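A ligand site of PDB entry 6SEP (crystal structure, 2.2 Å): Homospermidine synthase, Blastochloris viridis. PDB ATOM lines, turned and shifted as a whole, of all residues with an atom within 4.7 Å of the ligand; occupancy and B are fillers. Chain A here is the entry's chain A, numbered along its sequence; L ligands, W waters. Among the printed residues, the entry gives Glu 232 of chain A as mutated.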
ATOM      1  N   ILE A  20     -26.849  15.969 -32.168  1.00  0.00           N
ATOM      2  CA  ILE A  20     -26.824  15.563 -30.771  1.00  0.00           C
ATOM      3  C   ILE A  20     -27.364  16.727 -29.952  1.00  0.00           C
ATOM      4  O   ILE A  20     -26.738  17.794 -29.889  1.00  0.00           O
ATOM      5  CB  ILE A  20     -25.411  15.160 -30.331  1.00  0.00           C
ATOM      6  CG1 ILE A  20     -24.930  13.973 -31.173  1.00  0.00           C
ATOM      7  CG2 ILE A  20     -25.383  14.822 -28.847  1.00  0.00           C
ATOM      8  CD1 ILE A  20     -23.500  13.542 -30.903  1.00  0.00           C
ATOM      9  N   GLY A  21     -28.542  16.544 -29.365  1.00  0.00           N
ATOM     10  CA  GLY A  21     -29.173  17.592 -28.583  1.00  0.00           C
ATOM     11  C   GLY A  21     -30.157  18.393 -29.413  1.00  0.00           C
ATOM     12  O   GLY A  21     -29.802  18.924 -30.459  1.00  0.00           O
ATOM     13  N   PHE A  22     -31.405  18.483 -28.935  1.00  0.00           N
ATOM     14  CA  PHE A  22     -32.457  19.199 -29.643  1.00  0.00           C
ATOM     15  C   PHE A  22     -33.129  20.187 -28.684  1.00  0.00           C
ATOM     16  O   PHE A  22     -34.334  20.140 -28.427  1.00  0.00           O
ATOM     17  CB  PHE A  22     -33.467  18.219 -30.245  1.00  0.00           C
ATOM     18  CG  PHE A  22     -34.220  18.777 -31.417  1.00  0.00           C
ATOM     19  CD1 PHE A  22     -33.551  19.153 -32.572  1.00  0.00           C
ATOM     20  CD2 PHE A  22     -35.599  18.898 -31.386  1.00  0.00           C
ATOM     21  CE1 PHE A  22     -34.239  19.659 -33.656  1.00  0.00           C
ATOM     22  CE2 PHE A  22     -36.295  19.401 -32.466  1.00  0.00           C
ATOM     23  CZ  PHE A  22     -35.611  19.783 -33.604  1.00  0.00           C
ATOM     24  N   GLY A  23     -32.323  21.090 -28.138  1.00  0.00           N
ATOM     25  CA  GLY A  23     -32.799  22.165 -27.291  1.00  0.00           C
ATOM     26  C   GLY A  23     -33.102  23.412 -28.095  1.00  0.00           C
ATOM     27  O   GLY A  23     -33.408  23.358 -29.284  1.00  0.00           O
ATOM     28  N   SER A  24     -33.006  24.562 -27.422  1.00  0.00           N
ATOM     29  CA  SER A  24     -33.400  25.820 -28.055  1.00  0.00           C
ATOM     30  C   SER A  24     -32.609  26.070 -29.341  1.00  0.00           C
ATOM     31  O   SER A  24     -33.158  26.560 -30.327  1.00  0.00           O
ATOM     32  CB  SER A  24     -33.209  26.981 -27.070  1.00  0.00           C
ATOM     33  OG  SER A  24     -31.954  27.613 -27.234  1.00  0.00           O
ATOM     34  N   ILE A  25     -31.316  25.729 -29.348  1.00  0.00           N
ATOM     35  CA  ILE A  25     -30.489  25.975 -30.525  1.00  0.00           C
ATOM     36  C   ILE A  25     -30.732  24.910 -31.582  1.00  0.00           C
ATOM     37  O   ILE A  25     -30.766  25.220 -32.784  1.00  0.00           O
ATOM     38  CB  ILE A  25     -29.011  26.068 -30.131  1.00  0.00           C
ATOM     39  CG1 ILE A  25     -28.798  27.156 -29.072  1.00  0.00           C
ATOM     40  CG2 ILE A  25     -28.143  26.334 -31.356  1.00  0.00           C
ATOM     41  CD1 ILE A  25     -29.387  28.506 -29.449  1.00  0.00           C
ATOM     42  N   GLY A  26     -30.901  23.650 -31.179  1.00  0.00           N
ATOM     43  CA  GLY A  26     -31.202  22.608 -32.143  1.00  0.00           C
ATOM     44  C   GLY A  26     -32.526  22.851 -32.845  1.00  0.00           C
ATOM     45  O   GLY A  26     -32.649  22.628 -34.058  1.00  0.00           O
ATOM     46  N   ARG A  27     -33.539  23.299 -32.095  1.00  0.00           N
ATOM     47  CA  ARG A  27     -34.828  23.593 -32.704  1.00  0.00           C
ATOM     48  C   ARG A  27     -34.709  24.666 -33.773  1.00  0.00           C
ATOM     49  O   ARG A  27     -35.472  24.657 -34.747  1.00  0.00           O
ATOM     50  CB  ARG A  27     -35.832  24.021 -31.630  1.00  0.00           C
ATOM     51  CG  ARG A  27     -36.773  22.912 -31.156  1.00  0.00           C
ATOM     52  CD  ARG A  27     -36.329  22.245 -29.860  1.00  0.00           C
ATOM     53  NE  ARG A  27     -37.032  22.777 -28.692  1.00  0.00           N
ATOM     54  CZ  ARG A  27     -37.007  22.225 -27.490  1.00  0.00           C
ATOM     55  NH1 ARG A  27     -36.320  21.106 -27.260  1.00  0.00           N
ATOM     56  NH2 ARG A  27     -37.690  22.783 -26.494  1.00  0.00           N
ATOM     57  N   ILE A  47     -30.634  13.046 -31.493  1.00  0.00           N
ATOM     58  CA  ILE A  47     -30.371  12.301 -30.257  1.00  0.00           C
ATOM     59  C   ILE A  47     -30.534  13.260 -29.086  1.00  0.00           C
ATOM     60  O   ILE A  47     -29.884  14.306 -29.038  1.00  0.00           O
ATOM     61  CB  ILE A  47     -28.971  11.666 -30.271  1.00  0.00           C
ATOM     62  CG1 ILE A  47     -28.775  10.863 -31.561  1.00  0.00           C
ATOM     63  CG2 ILE A  47     -28.793  10.760 -29.066  1.00  0.00           C
ATOM     64  CD1 ILE A  47     -27.360  10.384 -31.765  1.00  0.00           C
ATOM     65  N   ASP A  48     -31.396  12.894 -28.139  1.00  0.00           N
ATOM     66  CA  ASP A  48     -31.692  13.728 -26.978  1.00  0.00           C
ATOM     67  C   ASP A  48     -32.455  12.888 -25.957  1.00  0.00           C
ATOM     68  O   ASP A  48     -33.308  12.096 -26.339  1.00  0.00           O
ATOM     69  CB  ASP A  48     -32.493  14.957 -27.391  1.00  0.00           C
ATOM     70  CG  ASP A  48     -32.622  15.983 -26.274  1.00  0.00           C
ATOM     71  OD1 ASP A  48     -33.078  15.624 -25.171  1.00  0.00           O
ATOM     72  OD2 ASP A  48     -32.275  17.160 -26.513  1.00  0.00           O
ATOM     73  N   PRO A  49     -32.169  13.012 -24.654  1.00  0.00           N
ATOM     74  CA  PRO A  49     -32.860  12.175 -23.675  1.00  0.00           C
ATOM     75  C   PRO A  49     -34.244  12.655 -23.265  1.00  0.00           C
ATOM     76  O   PRO A  49     -34.976  11.893 -22.618  1.00  0.00           O
ATOM     77  CB  PRO A  49     -31.924  12.209 -22.464  1.00  0.00           C
ATOM     78  CG  PRO A  49     -31.221  13.502 -22.578  1.00  0.00           C
ATOM     79  CD  PRO A  49     -31.038  13.741 -24.043  1.00  0.00           C
ATOM     80  N   SER A  50     -34.653  13.881 -23.612  1.00  0.00           N
ATOM     81  CA  SER A  50     -35.861  14.461 -23.058  1.00  0.00           C
ATOM     82  C   SER A  50     -37.095  14.064 -23.864  1.00  0.00           C
ATOM     83  O   SER A  50     -37.041  13.938 -25.092  1.00  0.00           O
ATOM     84  CB  SER A  50     -35.763  15.989 -23.017  1.00  0.00           C
ATOM     85  OG  SER A  50     -36.227  16.548 -24.231  1.00  0.00           O
ATOM     86  N   ALA A  53     -38.090  16.896 -26.305  1.00  0.00           N
ATOM     87  CA  ALA A  53     -37.391  16.884 -27.585  1.00  0.00           C
ATOM     88  C   ALA A  53     -37.982  15.835 -28.514  1.00  0.00           C
ATOM     89  O   ALA A  53     -38.096  16.068 -29.721  1.00  0.00           O
ATOM     90  CB  ALA A  53     -35.904  16.627 -27.364  1.00  0.00           C
ATOM     91  N   GLN A  67     -31.983   9.167 -26.057  1.00  0.00           N
ATOM     92  CA  GLN A  67     -30.826   8.615 -25.375  1.00  0.00           C
ATOM     93  C   GLN A  67     -29.917   9.767 -24.953  1.00  0.00           C
ATOM     94  O   GLN A  67     -29.777  10.748 -25.698  1.00  0.00           O
ATOM     95  CB  GLN A  67     -30.060   7.650 -26.281  1.00  0.00           C
ATOM     96  CG  GLN A  67     -29.118   6.710 -25.553  1.00  0.00           C
ATOM     97  CD  GLN A  67     -29.831   5.569 -24.836  1.00  0.00           C
ATOM     98  OE1 GLN A  67     -29.401   5.141 -23.760  1.00  0.00           O
ATOM     99  NE2 GLN A  67     -30.901   5.057 -25.429  1.00  0.00           N
ATOM    100  N   ALA A  68     -29.310   9.646 -23.782  1.00  0.00           N
ATOM    101  CA  ALA A  68     -28.293  10.577 -23.332  1.00  0.00           C
ATOM    102  C   ALA A  68     -26.934  10.045 -23.761  1.00  0.00           C
ATOM    103  O   ALA A  68     -26.574   8.909 -23.433  1.00  0.00           O
ATOM    104  CB  ALA A  68     -28.347  10.759 -21.820  1.00  0.00           C
ATOM    105  N   VAL A  69     -26.180  10.846 -24.515  1.00  0.00           N
ATOM    106  CA  VAL A  69     -24.837  10.467 -24.915  1.00  0.00           C
ATOM    107  C   VAL A  69     -23.923  10.564 -23.708  1.00  0.00           C
ATOM    108  O   VAL A  69     -23.747  11.647 -23.138  1.00  0.00           O
ATOM    109  CB  VAL A  69     -24.332  11.341 -26.061  1.00  0.00           C
ATOM    110  CG1 VAL A  69     -22.877  11.017 -26.371  1.00  0.00           C
ATOM    111  CG2 VAL A  69     -25.200  11.173 -27.300  1.00  0.00           C
ATOM    112  N   LEU A  94     -25.065  20.057 -30.433  1.00  0.00           N
ATOM    113  CA  LEU A  94     -25.731  21.188 -29.803  1.00  0.00           C
ATOM    114  C   LEU A  94     -26.340  20.759 -28.472  1.00  0.00           C
ATOM    115  O   LEU A  94     -27.511  21.032 -28.178  1.00  0.00           O
ATOM    116  CB  LEU A  94     -26.813  21.758 -30.723  1.00  0.00           C
ATOM    117  CG  LEU A  94     -26.355  22.196 -32.108  1.00  0.00           C
ATOM    118  CD1 LEU A  94     -27.558  22.558 -32.969  1.00  0.00           C
ATOM    119  CD2 LEU A  94     -25.399  23.373 -32.012  1.00  0.00           C
ATOM    120  N   SER A  95     -25.543  20.086 -27.661  1.00  0.00           N
ATOM    121  CA  SER A  95     -26.019  19.460 -26.437  1.00  0.00           C
ATOM    122  C   SER A  95     -25.294  20.046 -25.236  1.00  0.00           C
ATOM    123  O   SER A  95     -24.344  20.822 -25.361  1.00  0.00           O
ATOM    124  CB  SER A  95     -25.818  17.949 -26.483  1.00  0.00           C
ATOM    125  OG  SER A  95     -24.456  17.617 -26.695  1.00  0.00           O
ATOM    126  N   VAL A  96     -25.769  19.670 -24.055  1.00  0.00           N
ATOM    127  CA  VAL A  96     -25.058  19.882 -22.807  1.00  0.00           C
ATOM    128  C   VAL A  96     -24.642  18.523 -22.254  1.00  0.00           C
ATOM    129  O   VAL A  96     -25.068  17.474 -22.741  1.00  0.00           O
ATOM    130  CB  VAL A  96     -25.905  20.664 -21.779  1.00  0.00           C
ATOM    131  CG1 VAL A  96     -26.315  22.014 -22.352  1.00  0.00           C
ATOM    132  CG2 VAL A  96     -27.128  19.849 -21.365  1.00  0.00           C
ATOM    133  N   ASP A  97     -23.803  18.544 -21.228  1.00  0.00           N
ATOM    134  CA  ASP A  97     -23.415  17.358 -20.471  1.00  0.00           C
ATOM    135  C   ASP A  97     -22.618  16.348 -21.287  1.00  0.00           C
ATOM    136  O   ASP A  97     -22.414  15.221 -20.837  1.00  0.00           O
ATOM    137  CB  ASP A  97     -24.644  16.648 -19.881  1.00  0.00           C
ATOM    138  CG  ASP A  97     -25.425  17.533 -18.940  1.00  0.00           C
ATOM    139  OD1 ASP A  97     -24.836  18.500 -18.401  1.00  0.00           O
ATOM    140  OD2 ASP A  97     -26.631  17.265 -18.724  1.00  0.00           O
ATOM    141  N   THR A  98     -22.159  16.717 -22.485  1.00  0.00           N
ATOM    142  CA  THR A  98     -21.371  15.826 -23.335  1.00  0.00           C
ATOM    143  C   THR A  98     -19.981  16.408 -23.538  1.00  0.00           C
ATOM    144  O   THR A  98     -19.785  17.632 -23.508  1.00  0.00           O
ATOM    145  CB  THR A  98     -22.038  15.608 -24.699  1.00  0.00           C
ATOM    146  OG1 THR A  98     -22.159  16.860 -25.392  1.00  0.00           O
ATOM    147  CG2 THR A  98     -23.412  14.976 -24.550  1.00  0.00           C
ATOM    148  N   THR A 117     -20.761  24.396 -30.542  1.00  0.00           N
ATOM    149  CA  THR A 117     -20.789  25.805 -30.143  1.00  0.00           C
ATOM    150  C   THR A 117     -20.095  26.049 -28.803  1.00  0.00           C
ATOM    151  O   THR A 117     -20.124  27.173 -28.310  1.00  0.00           O
ATOM    152  CB  THR A 117     -22.230  26.309 -30.089  1.00  0.00           C
ATOM    153  OG1 THR A 117     -22.925  25.672 -29.016  1.00  0.00           O
ATOM    154  CG2 THR A 117     -22.951  26.013 -31.401  1.00  0.00           C
ATOM    155  N   VAL A 118     -19.477  25.036 -28.225  1.00  0.00           N
ATOM    156  CA  VAL A 118     -18.871  25.176 -26.905  1.00  0.00           C
ATOM    157  C   VAL A 118     -17.976  23.972 -26.628  1.00  0.00           C
ATOM    158  O   VAL A 118     -18.238  22.878 -27.112  1.00  0.00           O
ATOM    159  CB  VAL A 118     -19.944  25.328 -25.807  1.00  0.00           C
ATOM    160  CG1 VAL A 118     -20.846  24.092 -25.771  1.00  0.00           C
ATOM    161  CG2 VAL A 118     -19.306  25.568 -24.440  1.00  0.00           C
ATOM    162  N   GLU A 120     -17.633  21.608 -24.229  1.00  0.00           N
ATOM    163  CA  GLU A 120     -18.401  21.046 -23.133  1.00  0.00           C
ATOM    164  C   GLU A 120     -17.692  19.817 -22.566  1.00  0.00           C
ATOM    165  O   GLU A 120     -17.104  19.035 -23.321  1.00  0.00           O
ATOM    166  CB  GLU A 120     -19.803  20.661 -23.606  1.00  0.00           C
ATOM    167  CG  GLU A 120     -20.748  20.150 -22.514  1.00  0.00           C
ATOM    168  CD  GLU A 120     -21.365  21.267 -21.697  1.00  0.00           C
ATOM    169  OE1 GLU A 120     -20.977  22.437 -21.900  1.00  0.00           O
ATOM    170  OE2 GLU A 120     -22.253  20.975 -20.861  1.00  0.00           O
ATOM    171  N   GLY A 163     -20.718  29.314 -32.596  1.00  0.00           N
ATOM    172  CA  GLY A 163     -22.054  29.845 -32.407  1.00  0.00           C
ATOM    173  C   GLY A 163     -22.059  31.348 -32.629  1.00  0.00           C
ATOM    174  O   GLY A 163     -21.347  31.861 -33.492  1.00  0.00           O
ATOM    175  N   ALA A 164     -22.860  32.065 -31.838  1.00  0.00           N
ATOM    176  CA  ALA A 164     -22.814  33.529 -31.891  1.00  0.00           C
ATOM    177  C   ALA A 164     -21.597  34.059 -31.153  1.00  0.00           C
ATOM    178  O   ALA A 164     -20.838  34.875 -31.694  1.00  0.00           O
ATOM    179  CB  ALA A 164     -24.099  34.112 -31.301  1.00  0.00           C
ATOM    180  N   ASN A 165     -21.390  33.603 -29.928  1.00  0.00           N
ATOM    181  CA  ASN A 165     -20.237  34.004 -29.122  1.00  0.00           C
ATOM    182  C   ASN A 165     -19.968  32.916 -28.089  1.00  0.00           C
ATOM    183  O   ASN A 165     -20.717  32.792 -27.113  1.00  0.00           O
ATOM    184  CB  ASN A 165     -20.483  35.356 -28.454  1.00  0.00           C
ATOM    185  CG  ASN A 165     -21.825  35.435 -27.752  1.00  0.00           C
ATOM    186  OD1 ASN A 165     -22.771  34.726 -28.100  1.00  0.00           O
ATOM    187  ND2 ASN A 165     -21.918  36.304 -26.753  1.00  0.00           N
ATOM    188  N   PRO A 166     -18.913  32.105 -28.249  1.00  0.00           N
ATOM    189  CA  PRO A 166     -17.897  32.164 -29.314  1.00  0.00           C
ATOM    190  C   PRO A 166     -18.449  31.905 -30.708  1.00  0.00           C
ATOM    191  O   PRO A 166     -19.530  31.322 -30.848  1.00  0.00           O
ATOM    192  CB  PRO A 166     -16.915  31.060 -28.913  1.00  0.00           C
ATOM    193  CG  PRO A 166     -17.724  30.109 -28.115  1.00  0.00           C
ATOM    194  CD  PRO A 166     -18.695  30.952 -27.359  1.00  0.00           C
ATOM    195  N   GLU A 232     -31.737  31.702 -23.864  1.00  0.00           N
ATOM    196  CA  GLU A 232     -31.025  30.533 -24.362  1.00  0.00           C
ATOM    197  C   GLU A 232     -30.801  29.580 -23.194  1.00  0.00           C
ATOM    198  O   GLU A 232     -31.315  29.805 -22.089  1.00  0.00           O
ATOM    199  CB  GLU A 232     -29.718  30.957 -25.047  1.00  0.00           C
ATOM    200  CG  GLU A 232     -28.790  31.800 -24.181  1.00  0.00           C
ATOM    201  CD  GLU A 232     -27.642  32.412 -24.983  1.00  0.00           C
ATOM    202  OE1 GLU A 232     -26.798  33.114 -24.374  1.00  0.00           O
ATOM    203  OE2 GLU A 232     -27.599  32.210 -26.217  1.00  0.00           O
ATOM    204  N   SER A 233     -30.029  28.525 -23.437  1.00  0.00           N
ATOM    205  CA  SER A 233     -29.795  27.478 -22.452  1.00  0.00           C
ATOM    206  C   SER A 233     -29.624  28.043 -21.047  1.00  0.00           C
ATOM    207  O   SER A 233     -28.701  28.820 -20.780  1.00  0.00           O
ATOM    208  CB  SER A 233     -28.541  26.678 -22.831  1.00  0.00           C
ATOM    209  OG  SER A 233     -28.469  25.462 -22.118  1.00  0.00           O
ATOM    210  N   GLU A 235     -29.361  25.869 -18.259  1.00  0.00           N
ATOM    211  CA  GLU A 235     -28.338  25.001 -17.685  1.00  0.00           C
ATOM    212  C   GLU A 235     -26.950  25.419 -18.156  1.00  0.00           C
ATOM    213  O   GLU A 235     -26.021  25.525 -17.358  1.00  0.00           O
ATOM    214  CB  GLU A 235     -28.629  23.545 -18.066  1.00  0.00           C
ATOM    215  CG  GLU A 235     -30.020  23.084 -17.663  1.00  0.00           C
ATOM    216  CD  GLU A 235     -30.223  21.589 -17.870  1.00  0.00           C
ATOM    217  OE1 GLU A 235     -29.654  21.036 -18.836  1.00  0.00           O
ATOM    218  OE2 GLU A 235     -30.947  20.969 -17.065  1.00  0.00           O
ATOM    219  N   GLY A 236     -26.803  25.675 -19.452  1.00  0.00           N
ATOM    220  CA  GLY A 236     -25.508  26.094 -19.981  1.00  0.00           C
ATOM    221  C   GLY A 236     -25.065  27.438 -19.436  1.00  0.00           C
ATOM    222  O   GLY A 236     -23.895  27.626 -19.103  1.00  0.00           O
ATOM    223  N   ILE A 353     -37.021  28.799 -21.031  1.00  0.00           N
ATOM    224  CA  ILE A 353     -36.427  29.619 -22.093  1.00  0.00           C
ATOM    225  C   ILE A 353     -37.562  30.334 -22.809  1.00  0.00           C
ATOM    226  O   ILE A 353     -38.491  29.689 -23.306  1.00  0.00           O
ATOM    227  CB  ILE A 353     -35.602  28.767 -23.065  1.00  0.00           C
ATOM    228  CG1 ILE A 353     -34.473  28.042 -22.316  1.00  0.00           C
ATOM    229  CG2 ILE A 353     -35.024  29.640 -24.175  1.00  0.00           C
ATOM    230  CD1 ILE A 353     -33.683  27.070 -23.171  1.00  0.00           C
ATOM    231  N   VAL A 403     -27.190  32.461 -33.153  1.00  0.00           N
ATOM    232  CA  VAL A 403     -26.395  31.261 -32.922  1.00  0.00           C
ATOM    233  C   VAL A 403     -26.579  30.266 -34.053  1.00  0.00           C
ATOM    234  O   VAL A 403     -25.598  29.778 -34.643  1.00  0.00           O
ATOM    235  CB  VAL A 403     -26.758  30.642 -31.562  1.00  0.00           C
ATOM    236  CG1 VAL A 403     -25.918  29.408 -31.302  1.00  0.00           C
ATOM    237  CG2 VAL A 403     -26.605  31.660 -30.429  1.00  0.00           C
HETATM  238  P1  LIG L   1     -30.812  23.766 -24.039  1.00  0.00           P
HETATM  239  O1  LIG L   1     -32.031  24.490 -24.572  1.00  0.00           O
HETATM  240  O2  LIG L   1     -30.593  23.562 -22.562  1.00  0.00           O
HETATM  241  O3  LIG L   1     -30.769  22.338 -24.764  1.00  0.00           O
HETATM  242  C1  LIG L   1     -29.972  21.291 -24.220  1.00  0.00           C
HETATM  243  C2  LIG L   1     -30.410  19.986 -24.856  1.00  0.00           C
HETATM  244  O4  LIG L   1     -29.397  18.996 -24.667  1.00  0.00           O
HETATM  245  C3  LIG L   1     -31.696  19.462 -24.228  1.00  0.00           C
HETATM  246  O5  LIG L   1     -32.670  19.189 -25.235  1.00  0.00           O
HETATM  247  C4  LIG L   1     -31.272  18.202 -23.499  1.00  0.00           C
HETATM  248  O6  LIG L   1     -32.287  17.188 -23.528  1.00  0.00           O
HETATM  249  C5  LIG L   1     -30.024  17.781 -24.262  1.00  0.00           C
HETATM  250  N1  LIG L   1     -29.112  16.938 -23.475  1.00  0.00           N
HETATM  251  C6  LIG L   1     -28.840  17.025 -22.154  1.00  0.00           C
HETATM  252  N2  LIG L   1     -27.954  16.071 -21.781  1.00  0.00           N
HETATM  253  C7  LIG L   1     -27.652  15.353 -22.865  1.00  0.00           C
HETATM  254  C8  LIG L   1     -26.783  14.200 -23.168  1.00  0.00           C
HETATM  255  N3  LIG L   1     -26.057  13.635 -22.173  1.00  0.00           N
HETATM  256  N4  LIG L   1     -26.741  13.753 -24.436  1.00  0.00           N
HETATM  257  C9  LIG L   1     -27.474  14.320 -25.419  1.00  0.00           C
HETATM  258  N5  LIG L   1     -28.283  15.369 -25.215  1.00  0.00           N
HETATM  259  C10 LIG L   1     -28.411  15.926 -23.985  1.00  0.00           C
HETATM  260  O7  LIG L   1     -29.487  24.448 -24.639  1.00  0.00           O
HETATM  261  P2  LIG L   1     -29.433  25.231 -26.035  1.00  0.00           P
HETATM  262  O8  LIG L   1     -30.094  24.423 -27.125  1.00  0.00           O
HETATM  263  O9  LIG L   1     -29.872  26.659 -25.786  1.00  0.00           O
HETATM  264  O10 LIG L   1     -27.850  25.224 -26.273  1.00  0.00           O
HETATM  265  C11 LIG L   1     -27.161  24.046 -26.700  1.00  0.00           C
HETATM  266  C12 LIG L   1     -25.680  24.252 -26.424  1.00  0.00           C
HETATM  267  O11 LIG L   1     -25.228  25.368 -27.187  1.00  0.00           O
HETATM  268  C13 LIG L   1     -25.437  24.586 -24.952  1.00  0.00           C
HETATM  269  O12 LIG L   1     -24.460  23.690 -24.401  1.00  0.00           O
HETATM  270  C14 LIG L   1     -24.924  26.009 -24.926  1.00  0.00           C
HETATM  271  O13 LIG L   1     -23.820  26.160 -24.031  1.00  0.00           O
HETATM  272  C15 LIG L   1     -24.516  26.293 -26.365  1.00  0.00           C
HETATM  273  N6  LIG L   1     -24.783  27.669 -26.820  1.00  0.00           N
HETATM  274  C16 LIG L   1     -23.797  28.349 -27.418  1.00  0.00           C
HETATM  275  C17 LIG L   1     -23.985  29.648 -27.882  1.00  0.00           C
HETATM  276  C18 LIG L   1     -22.896  30.436 -28.552  1.00  0.00           C
HETATM  277  O14 LIG L   1     -23.171  31.534 -29.005  1.00  0.00           O
HETATM  278  N7  LIG L   1     -21.655  29.971 -28.671  1.00  0.00           N
HETATM  279  C19 LIG L   1     -25.233  30.233 -27.711  1.00  0.00           C
HETATM  280  C20 LIG L   1     -26.242  29.513 -27.093  1.00  0.00           C
HETATM  281  C21 LIG L   1     -26.000  28.212 -26.662  1.00  0.00           C
HETATM  282  O   HOH W   1     -32.628  17.023 -20.131  1.00  0.00           O
HETATM  283  O   HOH W   2     -29.958  22.414 -28.570  1.00  0.00           O
HETATM  284  O   HOH W   3     -34.371  23.531 -24.170  1.00  0.00           O
HETATM  285  O   HOH W   4     -29.652  18.316 -19.121  1.00  0.00           O
HETATM  286  O   HOH W   5     -21.493  28.615 -23.476  1.00  0.00           O
HETATM  287  O   HOH W   6     -27.586  14.782 -19.388  1.00  0.00           O
HETATM  288  O   HOH W   7     -26.061  12.828 -18.887  1.00  0.00           O
HETATM  289  O   HOH W   8     -31.795  24.959 -20.417  1.00  0.00           O
HETATM  290  O   HOH W   9     -31.262  21.745 -21.017  1.00  0.00           O
HETATM  291  O   HOH W  10     -24.574  28.462 -22.582  1.00  0.00           O
HETATM  292  O   HOH W  11     -23.475  12.827 -20.586  1.00  0.00           O
HETATM  293  O   HOH W  12     -22.710  24.621 -21.694  1.00  0.00           O
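OG of Ser 95 lies within hydrogen-bond range of OG1 of Thr 98, 2.7 Å away.
The backbone carbonyl oxygen (O) of Ile 20 sits at hydrogen-bond distance from the backbone NH (N) of Ser 95 (3.4 Å).
The side-chain hydroxyl of Ser 50 lies within hydrogen-bond range of the backbone NH of Ala 53, 2.8 Å away.
The backbone carbonyl oxygen (O) of Asp 48 sits at hydrogen-bond distance from the backbone NH (N) of Gln 67 (3.2 Å).
The backbone NH (N) of Gly 236 lies within hydrogen-bond range of the side-chain hydroxyl (OG) of Ser 233, at 3.2 Å.
The backbone carbonyl oxygen (O) of Phe 22 sits at hydrogen-bond distance from the guanidinium group (NH1) of Arg 27, 2.5 Å away.
OD1 of Asp 48 sits at hydrogen-bond distance from N of Ser 50 (2.8 Å).
N of Leu 94 sits at hydrogen-bond distance from O of Ile 20.
O of Val 96 lies close to N2 of the ligand, 3.3 Å away.
Phe 22 touches the ligand (C to O5, 3.6 Å).
CD of Pro 49 touches N5 of the ligand, at 3.4 Å.
Ser 50 touches the ligand.
CB of Ala 68 touches N3 of the ligand (3.7 Å).
Leu 94 touches the ligand (O to C11, 3.4 Å).
Asp 97 touches the ligand.
Thr 98 touches the ligand.
CG1 of Val 118 touches O12 of the ligand (3.9 Å).
CA of Gly 163 touches N7 of the ligand, at 3.8 Å.
Glu 232 touches the ligand (OE2 to C20, 3.1 Å).
Ile 353 touches the ligand (CD1 to O1, 3.4 Å).
Val 403 touches the ligand (CG2 to C19, 3.4 Å).
The backbone NH (N) of Gly 23 lies within hydrogen-bond range of an oxygen (O5) of the ligand (3.5 Å).
The side-chain amide oxygen (OD1) of Asn 165 lies close to an oxygen (O14) of the ligand, at 3.3 Å.
N of Ser 233 lies within hydrogen-bond range of O9 of the ligand, at 3.0 Å.
N7 of the ligand lies within hydrogen-bond range of O of Thr 117.
The backbone carbonyl oxygen (O) of Pro 166 is in hydrogen-bond range of a nitrogen (N7) of the ligand, 3.3 Å away.
O14 of the ligand is in hydrogen-bond range of N of Ala 164 (2.9 Å).
O14 of the ligand lies within hydrogen-bond range of N of Asn 165.
The backbone NH (N) of Ile 25 is in hydrogen-bond range of an oxygen (O8) of the ligand, at 2.9 Å.
N3 of the ligand sits at hydrogen-bond distance from O of Val 69, 3.2 Å away.
N of Ser 24 sits at hydrogen-bond distance from O8 of the ligand (2.9 Å).
An oxygen (O12) of the ligand lies within hydrogen-bond range of the backbone carbonyl oxygen (O) of Ser 95 (3.0 Å).
An oxygen (O11) of the ligand is in hydrogen-bond range of the side-chain hydroxyl of Thr 117, 3.0 Å away.
The side-chain hydroxyl (OG) of Ser 233 sits at hydrogen-bond distance from an oxygen (O2) of the ligand.
The backbone NH of Val 69 sits at hydrogen-bond distance from a nitrogen (N4) of the ligand, 3.0 Å away.
O9 of the ligand lies within hydrogen-bond range of OG of Ser 24, 2.7 Å away.
O of Asn 165 sits at hydrogen-bond distance from N7 of the ligand, 3.4 Å away.
An oxygen (O6) of the ligand sits at hydrogen-bond distance from the side-chain carboxylate (OD1) of Asp 48, 2.4 Å away.
Water W9 bridges an oxygen (O2) of the ligand (2.5 Å) and the side-chain carboxylate (OE1) of Glu 235 (2.8 Å).
Water W2 lies within hydrogen-bond range of O8 of the ligand, N of Gly 23, O of Leu 94 and N of Gly 26.
Water W6 lies within hydrogen-bond range of the side-chain carboxylate (OD2) of Asp 97 and a nitrogen (N2) of the ligand.
Water W8 lies within hydrogen-bond range of an oxygen (O2) of the ligand and the backbone NH (N) of Glu 235.
Water W12 lies within hydrogen-bond range of OE1 of Glu 120 and O13 of the ligand.
Water W4 bridges the side-chain carboxylate (OE1) of Glu 235 (2.7 Å) and the side-chain carboxylate (OD2) of Asp 97 (3.2 Å).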
